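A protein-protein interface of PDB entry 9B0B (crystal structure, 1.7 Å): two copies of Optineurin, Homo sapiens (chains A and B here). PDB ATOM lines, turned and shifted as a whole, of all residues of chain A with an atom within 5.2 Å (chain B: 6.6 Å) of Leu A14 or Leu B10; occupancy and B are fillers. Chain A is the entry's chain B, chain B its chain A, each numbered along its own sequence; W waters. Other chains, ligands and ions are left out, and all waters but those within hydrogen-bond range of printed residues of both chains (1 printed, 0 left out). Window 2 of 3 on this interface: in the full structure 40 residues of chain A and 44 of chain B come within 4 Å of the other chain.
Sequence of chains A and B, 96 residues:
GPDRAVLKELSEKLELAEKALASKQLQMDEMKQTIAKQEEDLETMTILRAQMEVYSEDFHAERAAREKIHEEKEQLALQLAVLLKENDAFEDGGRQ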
ATOM      1  N   LEU A   7     -18.707 -16.651  -9.058  1.00  0.00           N
ATOM      2  CA  LEU A   7     -19.005 -16.891 -10.458  1.00  0.00           C
ATOM      3  C   LEU A   7     -18.182 -18.070 -10.974  1.00  0.00           C
ATOM      4  O   LEU A   7     -18.668 -18.859 -11.789  1.00  0.00           O
ATOM      5  CB  LEU A   7     -18.717 -15.641 -11.291  1.00  0.00           C
ATOM      6  N   LEU A  10     -19.904 -21.451  -9.893  1.00  0.00           N
ATOM      7  CA  LEU A  10     -21.055 -21.705 -10.754  1.00  0.00           C
ATOM      8  C   LEU A  10     -20.611 -22.023 -12.175  1.00  0.00           C
ATOM      9  O   LEU A  10     -21.205 -22.867 -12.870  1.00  0.00           O
ATOM     10  CB  LEU A  10     -21.949 -20.468 -10.728  1.00  0.00           C
ATOM     11  CG  LEU A  10     -23.313 -20.507 -11.400  1.00  0.00           C
ATOM     12  CD1 LEU A  10     -24.078 -21.717 -10.906  1.00  0.00           C
ATOM     13  CD2 LEU A  10     -24.103 -19.233 -11.141  1.00  0.00           C
ATOM     14  N   SER A  11     -19.590 -21.309 -12.634  1.00  0.00           N
ATOM     15  CA  SER A  11     -18.955 -21.618 -13.895  1.00  0.00           C
ATOM     16  C   SER A  11     -18.456 -23.058 -13.912  1.00  0.00           C
ATOM     17  O   SER A  11     -18.614 -23.749 -14.925  1.00  0.00           O
ATOM     18  CB  SER A  11     -17.813 -20.644 -14.153  1.00  0.00           C
ATOM     19  OG  SER A  11     -17.417 -20.707 -15.509  1.00  0.00           O
ATOM     20  N   GLU A  12     -17.838 -23.517 -12.813  1.00  0.00           N
ATOM     21  CA  GLU A  12     -17.334 -24.886 -12.735  1.00  0.00           C
ATOM     22  C   GLU A  12     -18.469 -25.900 -12.792  1.00  0.00           C
ATOM     23  O   GLU A  12     -18.340 -26.957 -13.434  1.00  0.00           O
ATOM     24  CB  GLU A  12     -16.512 -25.088 -11.460  1.00  0.00           C
ATOM     25  CG  GLU A  12     -15.126 -24.428 -11.532  1.00  0.00           C
ATOM     26  CD  GLU A  12     -14.326 -24.553 -10.215  1.00  0.00           C
ATOM     27  OE1 GLU A  12     -14.853 -25.123  -9.231  1.00  0.00           O
ATOM     28  OE2 GLU A  12     -13.174 -24.064 -10.166  1.00  0.00           O
ATOM     29  N   LYS A  13     -19.572 -25.595 -12.107  1.00  0.00           N
ATOM     30  CA  LYS A  13     -20.731 -26.467 -12.100  1.00  0.00           C
ATOM     31  C   LYS A  13     -21.361 -26.552 -13.489  1.00  0.00           C
ATOM     32  O   LYS A  13     -21.806 -27.634 -13.919  1.00  0.00           O
ATOM     33  CB  LYS A  13     -21.764 -25.879 -11.159  1.00  0.00           C
ATOM     34  CG  LYS A  13     -22.990 -26.711 -10.943  1.00  0.00           C
ATOM     35  CD  LYS A  13     -22.967 -27.380  -9.576  1.00  0.00           C
ATOM     36  CE  LYS A  13     -24.206 -28.266  -9.378  1.00  0.00           C
ATOM     37  NZ  LYS A  13     -23.832 -29.700  -9.111  1.00  0.00           N
ATOM     38  N   LEU A  14     -21.438 -25.415 -14.177  1.00  0.00           N
ATOM     39  CA  LEU A  14     -22.026 -25.415 -15.520  1.00  0.00           C
ATOM     40  C   LEU A  14     -21.166 -26.223 -16.459  1.00  0.00           C
ATOM     41  O   LEU A  14     -21.680 -26.979 -17.298  1.00  0.00           O
ATOM     42  CB  LEU A  14     -22.202 -23.983 -16.023  1.00  0.00           C
ATOM     43  CG  LEU A  14     -22.491 -23.863 -17.502  1.00  0.00           C
ATOM     44  CD1 LEU A  14     -23.867 -24.496 -17.781  1.00  0.00           C
ATOM     45  CD2 LEU A  14     -22.551 -22.355 -17.923  1.00  0.00           C
ATOM     46  N   GLU A  15     -19.844 -26.083 -16.330  1.00  0.00           N
ATOM     47  CA  GLU A  15     -18.949 -26.817 -17.213  1.00  0.00           C
ATOM     48  C   GLU A  15     -19.095 -28.322 -16.979  1.00  0.00           C
ATOM     49  O   GLU A  15     -19.066 -29.114 -17.936  1.00  0.00           O
ATOM     50  CB  GLU A  15     -17.504 -26.378 -16.978  1.00  0.00           C
ATOM     51  CG  GLU A  15     -16.475 -27.087 -17.865  1.00  0.00           C
ATOM     52  CD  GLU A  15     -16.494 -26.611 -19.335  1.00  0.00           C
ATOM     53  OE1 GLU A  15     -17.200 -25.626 -19.676  1.00  0.00           O
ATOM     54  OE2 GLU A  15     -15.781 -27.230 -20.157  1.00  0.00           O
ATOM     55  N   LEU A  16     -19.205 -28.718 -15.723  1.00  0.00           N
ATOM     56  CA  LEU A  16     -19.438 -30.133 -15.460  1.00  0.00           C
ATOM     57  C   LEU A  16     -20.796 -30.585 -16.021  1.00  0.00           C
ATOM     58  O   LEU A  16     -20.946 -31.737 -16.482  1.00  0.00           O
ATOM     59  CB  LEU A  16     -19.350 -30.429 -13.962  1.00  0.00           C
ATOM     60  CG  LEU A  16     -17.911 -30.372 -13.381  1.00  0.00           C
ATOM     61  CD1 LEU A  16     -17.961 -30.691 -11.874  1.00  0.00           C
ATOM     62  CD2 LEU A  16     -16.979 -31.387 -14.041  1.00  0.00           C
ATOM     63  N   ALA A  17     -21.820 -29.742 -15.899  1.00  0.00           N
ATOM     64  CA  ALA A  17     -23.110 -30.140 -16.465  1.00  0.00           C
ATOM     65  C   ALA A  17     -22.984 -30.311 -17.974  1.00  0.00           C
ATOM     66  O   ALA A  17     -23.537 -31.257 -18.537  1.00  0.00           O
ATOM     67  CB  ALA A  17     -24.207 -29.119 -16.147  1.00  0.00           C
ATOM     68  N   GLU A  18     -22.240 -29.422 -18.638  1.00  0.00           N
ATOM     69  CA  GLU A  18     -22.097 -29.552 -20.095  1.00  0.00           C
ATOM     70  C   GLU A  18     -21.269 -30.771 -20.469  1.00  0.00           C
ATOM     71  O   GLU A  18     -21.537 -31.410 -21.486  1.00  0.00           O
ATOM     72  CB  GLU A  18     -21.511 -28.265 -20.693  1.00  0.00           C
ATOM     73  CG  GLU A  18     -22.484 -27.108 -20.611  1.00  0.00           C
ATOM     74  CD  GLU A  18     -22.036 -25.957 -21.522  1.00  0.00           C
ATOM     75  OE1 GLU A  18     -22.469 -25.927 -22.711  1.00  0.00           O
ATOM     76  OE2 GLU A  18     -21.197 -25.171 -21.073  1.00  0.00           O
ATOM     77  N   LYS A  19     -20.261 -31.136 -19.646  1.00  0.00           N
ATOM     78  CA  LYS A  19     -19.520 -32.358 -19.929  1.00  0.00           C
ATOM     79  C   LYS A  19     -20.378 -33.596 -19.736  1.00  0.00           C
ATOM     80  O   LYS A  19     -20.308 -34.521 -20.546  1.00  0.00           O
ATOM     81  CB  LYS A  19     -18.255 -32.440 -19.009  1.00  0.00           C
ATOM     82  CG  LYS A  19     -17.238 -31.396 -19.460  1.00  0.00           C
ATOM     83  CD  LYS A  19     -15.969 -31.383 -18.620  1.00  0.00           C
ATOM     84  CE  LYS A  19     -15.343 -32.761 -18.595  1.00  0.00           C
ATOM     85  NZ  LYS A  19     -14.558 -33.015 -19.849  1.00  0.00           N
ATOM     86  N   ALA B   5     -25.163  -9.493 -13.824  1.00  0.00           N
ATOM     87  CA  ALA B   5     -25.687  -9.965 -15.108  1.00  0.00           C
ATOM     88  C   ALA B   5     -24.961 -11.216 -15.590  1.00  0.00           C
ATOM     89  O   ALA B   5     -25.570 -12.059 -16.258  1.00  0.00           O
ATOM     90  CB  ALA B   5     -25.603  -8.879 -16.171  1.00  0.00           C
ATOM     91  N   VAL B   6     -23.669 -11.357 -15.272  1.00  0.00           N
ATOM     92  CA  VAL B   6     -22.958 -12.585 -15.613  1.00  0.00           C
ATOM     93  C   VAL B   6     -23.476 -13.710 -14.753  1.00  0.00           C
ATOM     94  O   VAL B   6     -23.548 -14.866 -15.183  1.00  0.00           O
ATOM     95  CB  VAL B   6     -21.441 -12.429 -15.436  1.00  0.00           C
ATOM     96  N   LEU B   7     -23.851 -13.384 -13.527  1.00  0.00           N
ATOM     97  CA  LEU B   7     -24.387 -14.368 -12.604  1.00  0.00           C
ATOM     98  C   LEU B   7     -25.776 -14.838 -13.025  1.00  0.00           C
ATOM     99  O   LEU B   7     -26.078 -16.037 -12.978  1.00  0.00           O
ATOM    100  CB  LEU B   7     -24.453 -13.740 -11.221  1.00  0.00           C
ATOM    101  CG  LEU B   7     -24.679 -14.664 -10.039  1.00  0.00           C
ATOM    102  CD1 LEU B   7     -26.172 -14.970  -9.829  1.00  0.00           C
ATOM    103  CD2 LEU B   7     -23.851 -15.916 -10.224  1.00  0.00           C
ATOM    104  N   LYS B   8     -26.643 -13.901 -13.406  1.00  0.00           N
ATOM    105  CA  LYS B   8     -27.952 -14.274 -13.916  1.00  0.00           C
ATOM    106  C   LYS B   8     -27.805 -15.165 -15.147  1.00  0.00           C
ATOM    107  O   LYS B   8     -28.515 -16.169 -15.296  1.00  0.00           O
ATOM    108  CB  LYS B   8     -28.755 -13.014 -14.235  1.00  0.00           C
ATOM    109  CG  LYS B   8     -30.080 -13.275 -14.905  1.00  0.00           C
ATOM    110  CD  LYS B   8     -31.104 -12.155 -14.653  1.00  0.00           C
ATOM    111  CE  LYS B   8     -32.103 -12.047 -15.799  1.00  0.00           C
ATOM    112  NZ  LYS B   8     -31.459 -11.614 -17.066  1.00  0.00           N
ATOM    113  N   GLU B   9     -26.882 -14.805 -16.042  1.00  0.00           N
ATOM    114  CA  GLU B   9     -26.668 -15.574 -17.262  1.00  0.00           C
ATOM    115  C   GLU B   9     -26.181 -16.982 -16.952  1.00  0.00           C
ATOM    116  O   GLU B   9     -26.630 -17.955 -17.581  1.00  0.00           O
ATOM    117  CB  GLU B   9     -25.671 -14.855 -18.166  1.00  0.00           C
ATOM    118  CG  GLU B   9     -26.294 -13.774 -19.012  1.00  0.00           C
ATOM    119  CD  GLU B   9     -25.245 -12.947 -19.709  1.00  0.00           C
ATOM    120  OE1 GLU B   9     -24.046 -13.251 -19.511  1.00  0.00           O
ATOM    121  OE2 GLU B   9     -25.613 -11.997 -20.437  1.00  0.00           O
ATOM    122  N   LEU B  10     -25.229 -17.108 -16.023  1.00  0.00           N
ATOM    123  CA  LEU B  10     -24.739 -18.427 -15.639  1.00  0.00           C
ATOM    124  C   LEU B  10     -25.849 -19.266 -15.017  1.00  0.00           C
ATOM    125  O   LEU B  10     -25.968 -20.468 -15.304  1.00  0.00           O
ATOM    126  CB  LEU B  10     -23.584 -18.298 -14.646  1.00  0.00           C
ATOM    127  CG  LEU B  10     -22.194 -17.919 -15.142  1.00  0.00           C
ATOM    128  CD1 LEU B  10     -21.253 -17.796 -13.931  1.00  0.00           C
ATOM    129  CD2 LEU B  10     -21.673 -18.958 -16.089  1.00  0.00           C
ATOM    130  N   SER B  11     -26.642 -18.665 -14.120  1.00  0.00           N
ATOM    131  CA  SER B  11     -27.703 -19.416 -13.458  1.00  0.00           C
ATOM    132  C   SER B  11     -28.740 -19.915 -14.461  1.00  0.00           C
ATOM    133  O   SER B  11     -29.219 -21.052 -14.356  1.00  0.00           O
ATOM    134  CB  SER B  11     -28.378 -18.555 -12.392  1.00  0.00           C
ATOM    135  OG  SER B  11     -27.400 -17.998 -11.548  1.00  0.00           O
ATOM    136  N   GLU B  12     -29.116 -19.067 -15.414  1.00  0.00           N
ATOM    137  CA  GLU B  12     -30.092 -19.485 -16.406  1.00  0.00           C
ATOM    138  C   GLU B  12     -29.541 -20.627 -17.261  1.00  0.00           C
ATOM    139  O   GLU B  12     -30.284 -21.539 -17.645  1.00  0.00           O
ATOM    140  CB  GLU B  12     -30.482 -18.314 -17.312  1.00  0.00           C
ATOM    141  CG  GLU B  12     -31.368 -17.280 -16.657  1.00  0.00           C
ATOM    142  CD  GLU B  12     -31.529 -16.033 -17.530  1.00  0.00           C
ATOM    143  OE1 GLU B  12     -30.793 -15.899 -18.535  1.00  0.00           O
ATOM    144  OE2 GLU B  12     -32.377 -15.177 -17.196  1.00  0.00           O
ATOM    145  N   LYS B  13     -28.263 -20.544 -17.629  1.00  0.00           N
ATOM    146  CA  LYS B  13     -27.685 -21.569 -18.491  1.00  0.00           C
ATOM    147  C   LYS B  13     -27.548 -22.873 -17.733  1.00  0.00           C
ATOM    148  O   LYS B  13     -27.771 -23.952 -18.297  1.00  0.00           O
ATOM    149  CB  LYS B  13     -26.350 -21.093 -19.055  1.00  0.00           C
ATOM    150  CG  LYS B  13     -25.757 -21.977 -20.084  1.00  0.00           C
ATOM    151  CD  LYS B  13     -24.824 -21.102 -20.957  1.00  0.00           C
ATOM    152  CE  LYS B  13     -24.108 -21.981 -21.956  1.00  0.00           C
ATOM    153  NZ  LYS B  13     -23.128 -21.243 -22.809  1.00  0.00           N
ATOM    154  N   LEU B  14     -27.213 -22.802 -16.443  1.00  0.00           N
ATOM    155  CA  LEU B  14     -27.134 -24.032 -15.668  1.00  0.00           C
ATOM    156  C   LEU B  14     -28.509 -24.696 -15.562  1.00  0.00           C
ATOM    157  O   LEU B  14     -28.629 -25.927 -15.657  1.00  0.00           O
ATOM    158  CB  LEU B  14     -26.528 -23.738 -14.284  1.00  0.00           C
ATOM    159  CG  LEU B  14     -26.636 -24.933 -13.346  1.00  0.00           C
ATOM    160  CD1 LEU B  14     -25.685 -25.988 -13.863  1.00  0.00           C
ATOM    161  CD2 LEU B  14     -26.220 -24.516 -11.927  1.00  0.00           C
ATOM    162  N   GLU B  15     -29.572 -23.901 -15.407  1.00  0.00           N
ATOM    163  CA  GLU B  15     -30.893 -24.516 -15.365  1.00  0.00           C
ATOM    164  C   GLU B  15     -31.273 -25.106 -16.718  1.00  0.00           C
ATOM    165  O   GLU B  15     -31.907 -26.169 -16.763  1.00  0.00           O
ATOM    166  CB  GLU B  15     -31.938 -23.503 -14.872  1.00  0.00           C
ATOM    167  CG  GLU B  15     -31.664 -23.090 -13.419  1.00  0.00           C
ATOM    168  CD  GLU B  15     -32.773 -22.269 -12.770  1.00  0.00           C
ATOM    169  OE1 GLU B  15     -33.893 -22.215 -13.317  1.00  0.00           O
ATOM    170  OE2 GLU B  15     -32.512 -21.668 -11.702  1.00  0.00           O
ATOM    171  N   ALA B  17     -29.076 -26.405 -18.764  1.00  0.00           N
ATOM    172  CA  ALA B  17     -28.313 -27.663 -18.810  1.00  0.00           C
ATOM    173  C   ALA B  17     -28.983 -28.780 -17.988  1.00  0.00           C
ATOM    174  O   ALA B  17     -28.994 -29.956 -18.407  1.00  0.00           O
ATOM    175  CB  ALA B  17     -26.881 -27.416 -18.328  1.00  0.00           C
HETATM  176  O   HOH W   1     -22.934 -23.760 -24.198  1.00  0.00           O
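Printed residues of chain B within 4 Å of Leu A7: Leu B10. Of the printed residues of chain B, Leu A10 touches Leu B7 (3.5 Å), Leu B10 (3.7 Å), Ser B11 (3.5 Å) and Leu B14 (3.7 Å). Leu A14 touches just these residues of chain B: Leu B10 (3.96 Å), Lys B13 (3.9 Å) and Leu B14 (3.9 Å). Leu A16 touches none of the printed residues of chain B. Lys A19 touches none of the printed residues of chain B. Printed residues of chain A within 4 Å of Leu B10: Leu A7 (3.5 Å), Leu A10 (3.7 Å) and Leu A14 (3.96 Å). Printed residues of chain A within 4 Å of Ser B11: Leu A10. Of the printed residues of chain A, Leu B14 touches Leu A10 (3.7 Å) and Leu A14 (3.9 Å).
Leu A7 touches Leu B10 (O to CD1, 3.5 Å). Leu B7 touches Leu A10 (CD2 to CD2, 3.5 Å). CB of Leu B10 touches CD2 of Leu A10, at 3.7 Å. OG of Ser B11 touches CD2 of Leu A10, 3.5 Å away. CD2 of Leu B14 touches CD1 of Leu A10 (3.7 Å). CD2 of Leu B10 touches CD2 of Leu A14, at 3.96 Å. Leu A14 touches Lys B13. CA of Leu B14 touches CD1 of Leu A14, at 3.9 Å. Ala A17 touches Ala B17.
The side-chain hydroxyl (OG) of Ser B11 is in hydrogen-bond range of the backbone carbonyl oxygen (O) of Leu B7 (2.8 Å).
Of the 12 printed residues of chain B, 6 touch a printed residue of chain A. Printed residues of chain B that touch a printed residue of chain A: Leu B7, Leu B10, Ser B11, Lys B13, Leu B14 and Ala B17. Of the 11 printed residues of chain A, 4 touch a printed residue of chain B. Printed residues of chain A that touch a printed residue of chain B: Leu A7, Leu A10, Leu A14 and Ala A17. Hydrophobic or aromatic side chains of chain A within 4 Å of the printed part of chain B: Leu A10, Leu A14 and Ala A17. Along chain A the printed residues that touch a printed residue of chain B span positions 7 to 17. Among the printed residues, 9 pairs touch across the chains. Among the printed residues, no Asp or Glu carboxylate lies within 4 Å of a Lys or Arg side-chain nitrogen of the other chain.
Water W1 bridges the side-chain carboxylate of Glu A18 (2.7 Å) and the side-chain amino group of Lys B13 (2.9 Å).
Leu A10 touches its own counterpart, Leu B10. Leu A10 touches Leu B14, and with the chains exchanged Leu A14 touches Leu B10. Leu A14 touches Lys B13, but with the chains exchanged Lys A13 does not touch Leu B14 (4.03 Å). Ala B17 touches its own counterpart, Ala A17. Positions printed for both chains: 7, 10, 11, 12, 13, 14, 15 and 17. Of the 9 pairs that touch across the chains among the printed residues, 7 have their exchanged pair printed and touching as well.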
